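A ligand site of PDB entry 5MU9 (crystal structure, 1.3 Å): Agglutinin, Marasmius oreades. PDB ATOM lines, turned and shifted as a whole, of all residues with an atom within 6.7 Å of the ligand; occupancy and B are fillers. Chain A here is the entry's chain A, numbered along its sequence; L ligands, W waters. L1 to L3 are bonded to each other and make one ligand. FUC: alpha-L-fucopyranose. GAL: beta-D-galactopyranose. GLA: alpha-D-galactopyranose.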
ATOM      1  N   HIS A   9      18.682  26.312 -27.094  1.00  0.00           N
ATOM      2  CA  HIS A   9      18.017  25.587 -26.039  1.00  0.00           C
ATOM      3  C   HIS A   9      18.483  24.135 -26.215  1.00  0.00           C
ATOM      4  O   HIS A   9      18.298  23.594 -27.312  1.00  0.00           O
ATOM      5  CB  HIS A   9      16.500  25.756 -26.254  1.00  0.00           C
ATOM      6  CG  HIS A   9      15.711  25.170 -25.148  1.00  0.00           C
ATOM      7  ND1 HIS A   9      14.976  24.003 -25.245  1.00  0.00           N
ATOM      8  CD2 HIS A   9      15.582  25.623 -23.885  1.00  0.00           C
ATOM      9  CE1 HIS A   9      14.457  23.759 -24.079  1.00  0.00           C
ATOM     10  NE2 HIS A   9      14.745  24.767 -23.268  1.00  0.00           N
ATOM     11  N   ASP A  20      19.813  23.420 -17.765  1.00  0.00           N
ATOM     12  CA  ASP A  20      19.244  24.532 -17.028  1.00  0.00           C
ATOM     13  C   ASP A  20      20.273  24.981 -15.996  1.00  0.00           C
ATOM     14  O   ASP A  20      20.756  24.181 -15.159  1.00  0.00           O
ATOM     15  CB  ASP A  20      17.947  24.046 -16.385  1.00  0.00           C
ATOM     16  CG  ASP A  20      17.173  25.137 -15.581  1.00  0.00           C
ATOM     17  OD1 ASP A  20      17.744  25.612 -14.588  1.00  0.00           O
ATOM     18  OD2 ASP A  20      15.990  25.377 -15.922  1.00  0.00           O
ATOM     19  N   LEU A  21      20.594  26.274 -15.961  1.00  0.00           N
ATOM     20  CA  LEU A  21      21.452  26.801 -14.888  1.00  0.00           C
ATOM     21  C   LEU A  21      20.553  27.128 -13.716  1.00  0.00           C
ATOM     22  O   LEU A  21      19.624  27.992 -13.798  1.00  0.00           O
ATOM     23  CB  LEU A  21      22.151  28.082 -15.380  1.00  0.00           C
ATOM     24  CG  LEU A  21      22.998  28.708 -14.316  1.00  0.00           C
ATOM     25  CD1 LEU A  21      24.203  27.865 -13.853  1.00  0.00           C
ATOM     26  CD2 LEU A  21      23.568  30.044 -14.837  1.00  0.00           C
ATOM     27  N   LYS A  22      20.700  26.395 -12.625  1.00  0.00           N
ATOM     28  CA  LYS A  22      19.707  26.374 -11.544  1.00  0.00           C
ATOM     29  C   LYS A  22      19.446  27.784 -10.984  1.00  0.00           C
ATOM     30  O   LYS A  22      20.347  28.456 -10.521  1.00  0.00           O
ATOM     31  CB  LYS A  22      20.113  25.388 -10.449  1.00  0.00           C
ATOM     32  CG  LYS A  22      18.920  24.963  -9.665  1.00  0.00           C
ATOM     33  CD  LYS A  22      19.260  23.821  -8.643  1.00  0.00           C
ATOM     34  CE  LYS A  22      18.010  23.443  -7.888  1.00  0.00           C
ATOM     35  NZ  LYS A  22      18.258  22.261  -6.973  1.00  0.00           N
ATOM     36  N   ASP A  23      18.158  28.131 -11.007  1.00  0.00           N
ATOM     37  CA  ASP A  23      17.675  29.457 -10.569  1.00  0.00           C
ATOM     38  C   ASP A  23      18.256  30.617 -11.359  1.00  0.00           C
ATOM     39  O   ASP A  23      18.139  31.794 -10.902  1.00  0.00           O
ATOM     40  CB  ASP A  23      17.867  29.663  -9.046  1.00  0.00           C
ATOM     41  CG  ASP A  23      16.869  30.647  -8.426  1.00  0.00           C
ATOM     42  OD1 ASP A  23      15.713  30.632  -8.860  1.00  0.00           O
ATOM     43  OD2 ASP A  23      17.269  31.424  -7.497  1.00  0.00           O
ATOM     44  N   GLY A  24      18.910  30.327 -12.479  1.00  0.00           N
ATOM     45  CA  GLY A  24      19.594  31.383 -13.213  1.00  0.00           C
ATOM     46  C   GLY A  24      20.733  32.058 -12.453  1.00  0.00           C
ATOM     47  O   GLY A  24      21.116  33.148 -12.828  1.00  0.00           O
ATOM     48  N   VAL A  33      21.685  21.616 -14.384  1.00  0.00           N
ATOM     49  CA  VAL A  33      20.744  20.485 -14.126  1.00  0.00           C
ATOM     50  C   VAL A  33      19.824  20.252 -15.283  1.00  0.00           C
ATOM     51  O   VAL A  33      19.561  21.158 -16.104  1.00  0.00           O
ATOM     52  CB  VAL A  33      19.968  20.673 -12.816  1.00  0.00           C
ATOM     53  CG1 VAL A  33      20.904  20.741 -11.583  1.00  0.00           C
ATOM     54  CG2 VAL A  33      19.093  21.949 -12.895  1.00  0.00           C
ATOM     55  N   TRP A  35      15.989  19.987 -16.578  1.00  0.00           N
ATOM     56  CA  TRP A  35      14.695  20.603 -16.106  1.00  0.00           C
ATOM     57  C   TRP A  35      13.728  20.609 -17.280  1.00  0.00           C
ATOM     58  O   TRP A  35      14.105  20.871 -18.425  1.00  0.00           O
ATOM     59  CB  TRP A  35      14.988  22.044 -15.598  1.00  0.00           C
ATOM     60  CG  TRP A  35      13.985  22.579 -14.601  1.00  0.00           C
ATOM     61  CD1 TRP A  35      12.690  23.005 -14.797  1.00  0.00           C
ATOM     62  CD2 TRP A  35      14.210  22.628 -13.206  1.00  0.00           C
ATOM     63  NE1 TRP A  35      12.071  23.332 -13.585  1.00  0.00           N
ATOM     64  CE2 TRP A  35      12.997  23.114 -12.600  1.00  0.00           C
ATOM     65  CE3 TRP A  35      15.288  22.334 -12.381  1.00  0.00           C
ATOM     66  CZ2 TRP A  35      12.915  23.285 -11.205  1.00  0.00           C
ATOM     67  CZ3 TRP A  35      15.164  22.450 -11.048  1.00  0.00           C
ATOM     68  CH2 TRP A  35      14.034  22.966 -10.482  1.00  0.00           C
ATOM     69  N   GLN A  36      12.463  20.424 -16.977  1.00  0.00           N
ATOM     70  CA  GLN A  36      11.408  20.494 -18.033  1.00  0.00           C
ATOM     71  C   GLN A  36      11.297  21.884 -18.544  1.00  0.00           C
ATOM     72  O   GLN A  36      11.724  22.913 -17.933  1.00  0.00           O
ATOM     73  CB  GLN A  36      10.121  19.953 -17.488  1.00  0.00           C
ATOM     74  CG  GLN A  36       9.387  20.839 -16.433  1.00  0.00           C
ATOM     75  CD  GLN A  36       8.129  20.243 -15.981  1.00  0.00           C
ATOM     76  OE1 GLN A  36       7.205  20.082 -16.769  1.00  0.00           O
ATOM     77  NE2 GLN A  36       8.112  19.836 -14.725  1.00  0.00           N
ATOM     78  N   PHE A  37      10.659  22.008 -19.723  1.00  0.00           N
ATOM     79  CA  PHE A  37      10.561  23.287 -20.411  1.00  0.00           C
ATOM     80  C   PHE A  37       9.224  23.434 -21.073  1.00  0.00           C
ATOM     81  O   PHE A  37       8.432  22.456 -21.177  1.00  0.00           O
ATOM     82  CB  PHE A  37      11.685  23.384 -21.448  1.00  0.00           C
ATOM     83  CG  PHE A  37      11.634  22.385 -22.546  1.00  0.00           C
ATOM     84  CD1 PHE A  37      12.286  21.174 -22.462  1.00  0.00           C
ATOM     85  CD2 PHE A  37      10.992  22.699 -23.736  1.00  0.00           C
ATOM     86  CE1 PHE A  37      12.277  20.292 -23.471  1.00  0.00           C
ATOM     87  CE2 PHE A  37      10.987  21.776 -24.752  1.00  0.00           C
ATOM     88  CZ  PHE A  37      11.635  20.610 -24.588  1.00  0.00           C
ATOM     89  N   THR A  38       8.928  24.681 -21.536  1.00  0.00           N
ATOM     90  CA  THR A  38       7.643  24.919 -22.209  1.00  0.00           C
ATOM     91  C   THR A  38       8.013  25.376 -23.616  1.00  0.00           C
ATOM     92  O   THR A  38       8.694  26.435 -23.789  1.00  0.00           O
ATOM     93  CB  THR A  38       6.800  25.995 -21.455  1.00  0.00           C
ATOM     94  OG1 THR A  38       6.654  25.612 -20.081  1.00  0.00           O
ATOM     95  CG2 THR A  38       5.493  26.150 -22.151  1.00  0.00           C
ATOM     96  N   PRO A  39       7.593  24.701 -24.670  1.00  0.00           N
ATOM     97  CA  PRO A  39       7.900  25.118 -26.031  1.00  0.00           C
ATOM     98  C   PRO A  39       7.257  26.446 -26.347  1.00  0.00           C
ATOM     99  O   PRO A  39       6.260  26.787 -25.745  1.00  0.00           O
ATOM    100  CB  PRO A  39       7.292  24.046 -26.951  1.00  0.00           C
ATOM    101  CG  PRO A  39       7.187  22.857 -26.003  1.00  0.00           C
ATOM    102  CD  PRO A  39       6.824  23.419 -24.667  1.00  0.00           C
ATOM    103  N   THR A  41       8.096  29.445 -25.649  1.00  0.00           N
ATOM    104  CA  THR A  41       8.352  30.458 -24.577  1.00  0.00           C
ATOM    105  C   THR A  41       9.825  30.826 -24.580  1.00  0.00           C
ATOM    106  O   THR A  41      10.692  30.105 -25.106  1.00  0.00           O
ATOM    107  CB  THR A  41       7.940  29.938 -23.199  1.00  0.00           C
ATOM    108  OG1 THR A  41       8.892  28.990 -22.710  1.00  0.00           O
ATOM    109  CG2 THR A  41       6.507  29.435 -23.136  1.00  0.00           C
ATOM    110  N   ILE A  42      10.153  31.938 -23.888  1.00  0.00           N
ATOM    111  CA  ILE A  42      11.464  32.113 -23.365  1.00  0.00           C
ATOM    112  C   ILE A  42      11.630  31.290 -22.107  1.00  0.00           C
ATOM    113  O   ILE A  42      10.965  31.485 -21.079  1.00  0.00           O
ATOM    114  CB  ILE A  42      11.748  33.629 -23.092  1.00  0.00           C
ATOM    115  CG1 ILE A  42      11.706  34.451 -24.418  1.00  0.00           C
ATOM    116  CG2 ILE A  42      13.066  33.776 -22.367  1.00  0.00           C
ATOM    117  CD1 ILE A  42      12.708  34.123 -25.478  1.00  0.00           C
ATOM    118  N   ASN A  43      12.544  30.295 -22.210  1.00  0.00           N
ATOM    119  CA  ASN A  43      12.875  29.451 -21.050  1.00  0.00           C
ATOM    120  C   ASN A  43      14.089  30.109 -20.444  1.00  0.00           C
ATOM    121  O   ASN A  43      15.256  29.924 -20.860  1.00  0.00           O
ATOM    122  CB  ASN A  43      13.151  28.019 -21.479  1.00  0.00           C
ATOM    123  CG  ASN A  43      11.896  27.281 -21.894  1.00  0.00           C
ATOM    124  OD1 ASN A  43      11.129  26.882 -21.041  1.00  0.00           O
ATOM    125  ND2 ASN A  43      11.694  27.129 -23.173  1.00  0.00           N
ATOM    126  N   TRP A  44      13.820  30.964 -19.441  1.00  0.00           N
ATOM    127  CA  TRP A  44      14.732  31.960 -18.919  1.00  0.00           C
ATOM    128  C   TRP A  44      16.120  31.474 -18.423  1.00  0.00           C
ATOM    129  O   TRP A  44      17.102  32.204 -18.544  1.00  0.00           O
ATOM    130  CB  TRP A  44      14.058  32.773 -17.770  1.00  0.00           C
ATOM    131  CG  TRP A  44      13.115  33.780 -18.301  1.00  0.00           C
ATOM    132  CD1 TRP A  44      11.801  33.647 -18.453  1.00  0.00           C
ATOM    133  CD2 TRP A  44      13.450  35.082 -18.794  1.00  0.00           C
ATOM    134  NE1 TRP A  44      11.255  34.775 -18.970  1.00  0.00           N
ATOM    135  CE2 TRP A  44      12.252  35.666 -19.241  1.00  0.00           C
ATOM    136  CE3 TRP A  44      14.617  35.766 -18.902  1.00  0.00           C
ATOM    137  CZ2 TRP A  44      12.210  36.927 -19.757  1.00  0.00           C
ATOM    138  CZ3 TRP A  44      14.601  36.977 -19.428  1.00  0.00           C
ATOM    139  CH2 TRP A  44      13.431  37.582 -19.868  1.00  0.00           C
ATOM    140  N   HIS A  45      16.202  30.227 -17.865  1.00  0.00           N
ATOM    141  CA  HIS A  45      17.411  29.739 -17.326  1.00  0.00           C
ATOM    142  C   HIS A  45      18.109  28.698 -18.270  1.00  0.00           C
ATOM    143  O   HIS A  45      19.119  28.097 -17.855  1.00  0.00           O
ATOM    144  CB  HIS A  45      17.199  29.125 -15.939  1.00  0.00           C
ATOM    145  CG  HIS A  45      16.572  30.086 -15.012  1.00  0.00           C
ATOM    146  ND1 HIS A  45      15.886  29.674 -13.896  1.00  0.00           N
ATOM    147  CD2 HIS A  45      16.543  31.441 -14.967  1.00  0.00           C
ATOM    148  CE1 HIS A  45      15.449  30.716 -13.211  1.00  0.00           C
ATOM    149  NE2 HIS A  45      15.833  31.820 -13.846  1.00  0.00           N
ATOM    150  N   GLN A  46      17.561  28.560 -19.503  1.00  0.00           N
ATOM    151  CA  GLN A  46      17.897  27.415 -20.367  1.00  0.00           C
ATOM    152  C   GLN A  46      18.412  27.868 -21.733  1.00  0.00           C
ATOM    153  O   GLN A  46      18.318  27.098 -22.678  1.00  0.00           O
ATOM    154  CB  GLN A  46      16.657  26.523 -20.520  1.00  0.00           C
ATOM    155  CG  GLN A  46      16.120  25.966 -19.208  1.00  0.00           C
ATOM    156  CD  GLN A  46      14.860  25.124 -19.337  1.00  0.00           C
ATOM    157  OE1 GLN A  46      14.272  25.034 -20.439  1.00  0.00           O
ATOM    158  NE2 GLN A  46      14.362  24.608 -18.203  1.00  0.00           N
ATOM    159  N   PHE A  66      21.058  34.302 -19.488  1.00  0.00           N
ATOM    160  CA  PHE A  66      20.563  35.050 -18.336  1.00  0.00           C
ATOM    161  C   PHE A  66      21.653  35.439 -17.325  1.00  0.00           C
ATOM    162  O   PHE A  66      21.715  36.635 -16.953  1.00  0.00           O
ATOM    163  CB  PHE A  66      19.440  34.249 -17.668  1.00  0.00           C
ATOM    164  CG  PHE A  66      18.837  34.958 -16.461  1.00  0.00           C
ATOM    165  CD1 PHE A  66      17.889  35.962 -16.682  1.00  0.00           C
ATOM    166  CD2 PHE A  66      19.182  34.630 -15.210  1.00  0.00           C
ATOM    167  CE1 PHE A  66      17.310  36.622 -15.622  1.00  0.00           C
ATOM    168  CE2 PHE A  66      18.561  35.241 -14.108  1.00  0.00           C
ATOM    169  CZ  PHE A  66      17.683  36.268 -14.320  1.00  0.00           C
ATOM    170  N   ASP A 131      12.989  17.291 -12.433  1.00  0.00           N
ATOM    171  CA  ASP A 131      13.480  18.657 -12.426  1.00  0.00           C
ATOM    172  C   ASP A 131      14.605  18.766 -11.421  1.00  0.00           C
ATOM    173  O   ASP A 131      14.376  18.454 -10.169  1.00  0.00           O
ATOM    174  CB  ASP A 131      12.389  19.651 -12.103  1.00  0.00           C
ATOM    175  CG  ASP A 131      11.296  19.675 -13.241  1.00  0.00           C
ATOM    176  OD1 ASP A 131      11.629  19.426 -14.372  1.00  0.00           O
ATOM    177  OD2 ASP A 131      10.139  20.147 -12.900  1.00  0.00           O
HETATM  178  C1  FUC L   1      10.202  29.701 -14.548  1.00  0.00           C
HETATM  179  C2  FUC L   1       8.788  30.098 -14.173  1.00  0.00           C
HETATM  180  C3  FUC L   1       8.833  31.202 -13.145  1.00  0.00           C
HETATM  181  C4  FUC L   1       9.644  32.368 -13.609  1.00  0.00           C
HETATM  182  C5  FUC L   1      11.063  31.833 -13.944  1.00  0.00           C
HETATM  183  C6  FUC L   1      12.003  32.901 -14.408  1.00  0.00           C
HETATM  184  O2  FUC L   1       8.089  28.920 -13.624  1.00  0.00           O
HETATM  185  O3  FUC L   1       7.425  31.604 -12.862  1.00  0.00           O
HETATM  186  O4  FUC L   1       9.058  33.028 -14.718  1.00  0.00           O
HETATM  187  O5  FUC L   1      10.968  30.848 -14.962  1.00  0.00           O
HETATM  188  C1  GAL L   2      12.639  28.548 -12.227  1.00  0.00           C
HETATM  189  C2  GAL L   2      12.119  28.570 -13.658  1.00  0.00           C
HETATM  190  C3  GAL L   2      12.167  27.184 -14.239  1.00  0.00           C
HETATM  191  C4  GAL L   2      13.522  26.554 -14.119  1.00  0.00           C
HETATM  192  C5  GAL L   2      13.985  26.614 -12.645  1.00  0.00           C
HETATM  193  C6  GAL L   2      15.380  26.064 -12.383  1.00  0.00           C
HETATM  194  O1  GAL L   2      12.790  29.861 -11.783  1.00  0.00           O
HETATM  195  O2  GAL L   2      10.752  28.996 -13.489  1.00  0.00           O
HETATM  196  O3  GAL L   2      11.662  27.313 -15.557  1.00  0.00           O
HETATM  197  O4  GAL L   2      14.454  27.219 -14.970  1.00  0.00           O
HETATM  198  O5  GAL L   2      13.957  28.012 -12.206  1.00  0.00           O
HETATM  199  O6  GAL L   2      16.396  26.953 -12.868  1.00  0.00           O
HETATM  200  C1  GLA L   3      11.575  26.073 -16.308  1.00  0.00           C
HETATM  201  C2  GLA L   3      10.967  26.316 -17.683  1.00  0.00           C
HETATM  202  C3  GLA L   3       9.479  26.613 -17.615  1.00  0.00           C
HETATM  203  C4  GLA L   3       8.743  25.580 -16.814  1.00  0.00           C
HETATM  204  C5  GLA L   3       9.413  25.539 -15.432  1.00  0.00           C
HETATM  205  C6  GLA L   3       8.804  24.549 -14.461  1.00  0.00           C
HETATM  206  O2  GLA L   3      11.631  27.374 -18.381  1.00  0.00           O
HETATM  207  O3  GLA L   3       8.891  26.670 -18.922  1.00  0.00           O
HETATM  208  O4  GLA L   3       8.833  24.272 -17.448  1.00  0.00           O
HETATM  209  O5  GLA L   3      10.770  25.132 -15.605  1.00  0.00           O
HETATM  210  O6  GLA L   3       9.446  24.572 -13.174  1.00  0.00           O
HETATM  211  O   HOH W   1       9.074  27.010 -11.794  1.00  0.00           O
HETATM  212  O   HOH W   2       9.383  22.406 -11.495  1.00  0.00           O
HETATM  213  O   HOH W   3      14.595  28.174  -9.427  1.00  0.00           O
HETATM  214  O   HOH W   4      14.065  28.414 -17.436  1.00  0.00           O
HETATM  215  O   HOH W   5       8.911  31.774 -17.194  1.00  0.00           O
HETATM  216  O   HOH W   6       7.529  34.278 -11.763  1.00  0.00           O
HETATM  217  O   HOH W   7      11.091  30.329 -18.170  1.00  0.00           O
HETATM  218  O   HOH W   8       9.149  29.181 -19.948  1.00  0.00           O
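Water W8 lies within hydrogen-bond range of an oxygen (O3) of GLA L3, the side-chain hydroxyl of Thr 41, the backbone carbonyl oxygen of Ile 42 and the side-chain amide oxygen of Asn 43. Water W2 lies within hydrogen-bond range of O6 of GLA L3 and OD2 of Asp 131. Water W4 lies within hydrogen-bond range of O4 of GAL L2 (2.8 Å), N of His 45 (2.8 Å) and N of Trp 44 (3.3 Å). Water W3 bridges the side-chain carboxylate (OD1) of Asp 23 and an oxygen (O5) of GAL L2. Water W7 lies within hydrogen-bond range of O2 of GLA L3 (3.0 Å), N of Trp 44 (3.1 Å) and O of Ile 42 (3.1 Å).
A ring nitrogen (ND1) of His 45 sits at hydrogen-bond distance from an oxygen (O6) of GAL L2, at 3.0 Å. An oxygen (O6) of GAL L2 sits at hydrogen-bond distance from the side-chain carboxylate (OD1) of Asp 20, 2.6 Å away. O of Gln 36 is in hydrogen-bond range of O4 of GLA L3, 3.2 Å away. The indole nitrogen (NE1) of Trp 35 is in hydrogen-bond range of an oxygen (O6) of GLA L3 (2.9 Å). An oxygen (O3) of GLA L3 sits at hydrogen-bond distance from the side-chain hydroxyl (OG1) of Thr 38 (2.7 Å). An oxygen (O2) of GLA L3 lies within hydrogen-bond range of the side-chain amide oxygen (OD1) of Asn 43 (2.8 Å). The backbone NH of Thr 38 lies within hydrogen-bond range of an oxygen (O3) of GLA L3 (3.3 Å). An oxygen (O6) of GAL L2 sits at hydrogen-bond distance from the backbone NH (N) of Asp 23 (2.8 Å).
The side-chain amide nitrogen (NE2) of Gln 46 sits at hydrogen-bond distance from the backbone carbonyl oxygen (O) of Gln 36 (3.1 Å). O of His 45 lies within hydrogen-bond range of N of Leu 21 (3.0 Å). The side-chain amide nitrogen of Gln 36 lies within hydrogen-bond range of the side-chain carboxylate of Asp 131 (2.7 Å). ND1 of His 45 sits at hydrogen-bond distance from N of Gly 24, 3.4 Å away. The side-chain carboxylate (OD2) of Asp 20 lies within hydrogen-bond range of the side-chain amide nitrogen (NE2) of Gln 46 (2.9 Å). ND2 of Asn 43 sits at hydrogen-bond distance from O of Thr 38 (3.1 Å). The side-chain amide oxygen of Gln 46 is in hydrogen-bond range of a ring nitrogen (NE2) of His 9, at 2.9 Å. O of Thr 38 sits at hydrogen-bond distance from OG1 of Thr 41 (2.8 Å).
O of Leu 21 touches O6 of GAL L2 (3.5 Å). CA of Lys 22 touches O6 of GAL L2 (3.6 Å). CA of Phe 37 touches O4 of GLA L3, 3.6 Å away. CB of Trp 44 touches C6 of FUC L1 (3.9 Å). NE2 of Gln 46 touches C1 of GLA L3, 3.7 Å away. Hydrophobic or aromatic side chains that line the ligand: Trp 35, Trp 44 and His 45. Of the 20 residues printed, 12 come within 4 Å of the ligand. The nearest printed residue that does not touch the ligand is Gly 24 (4.2 Å).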
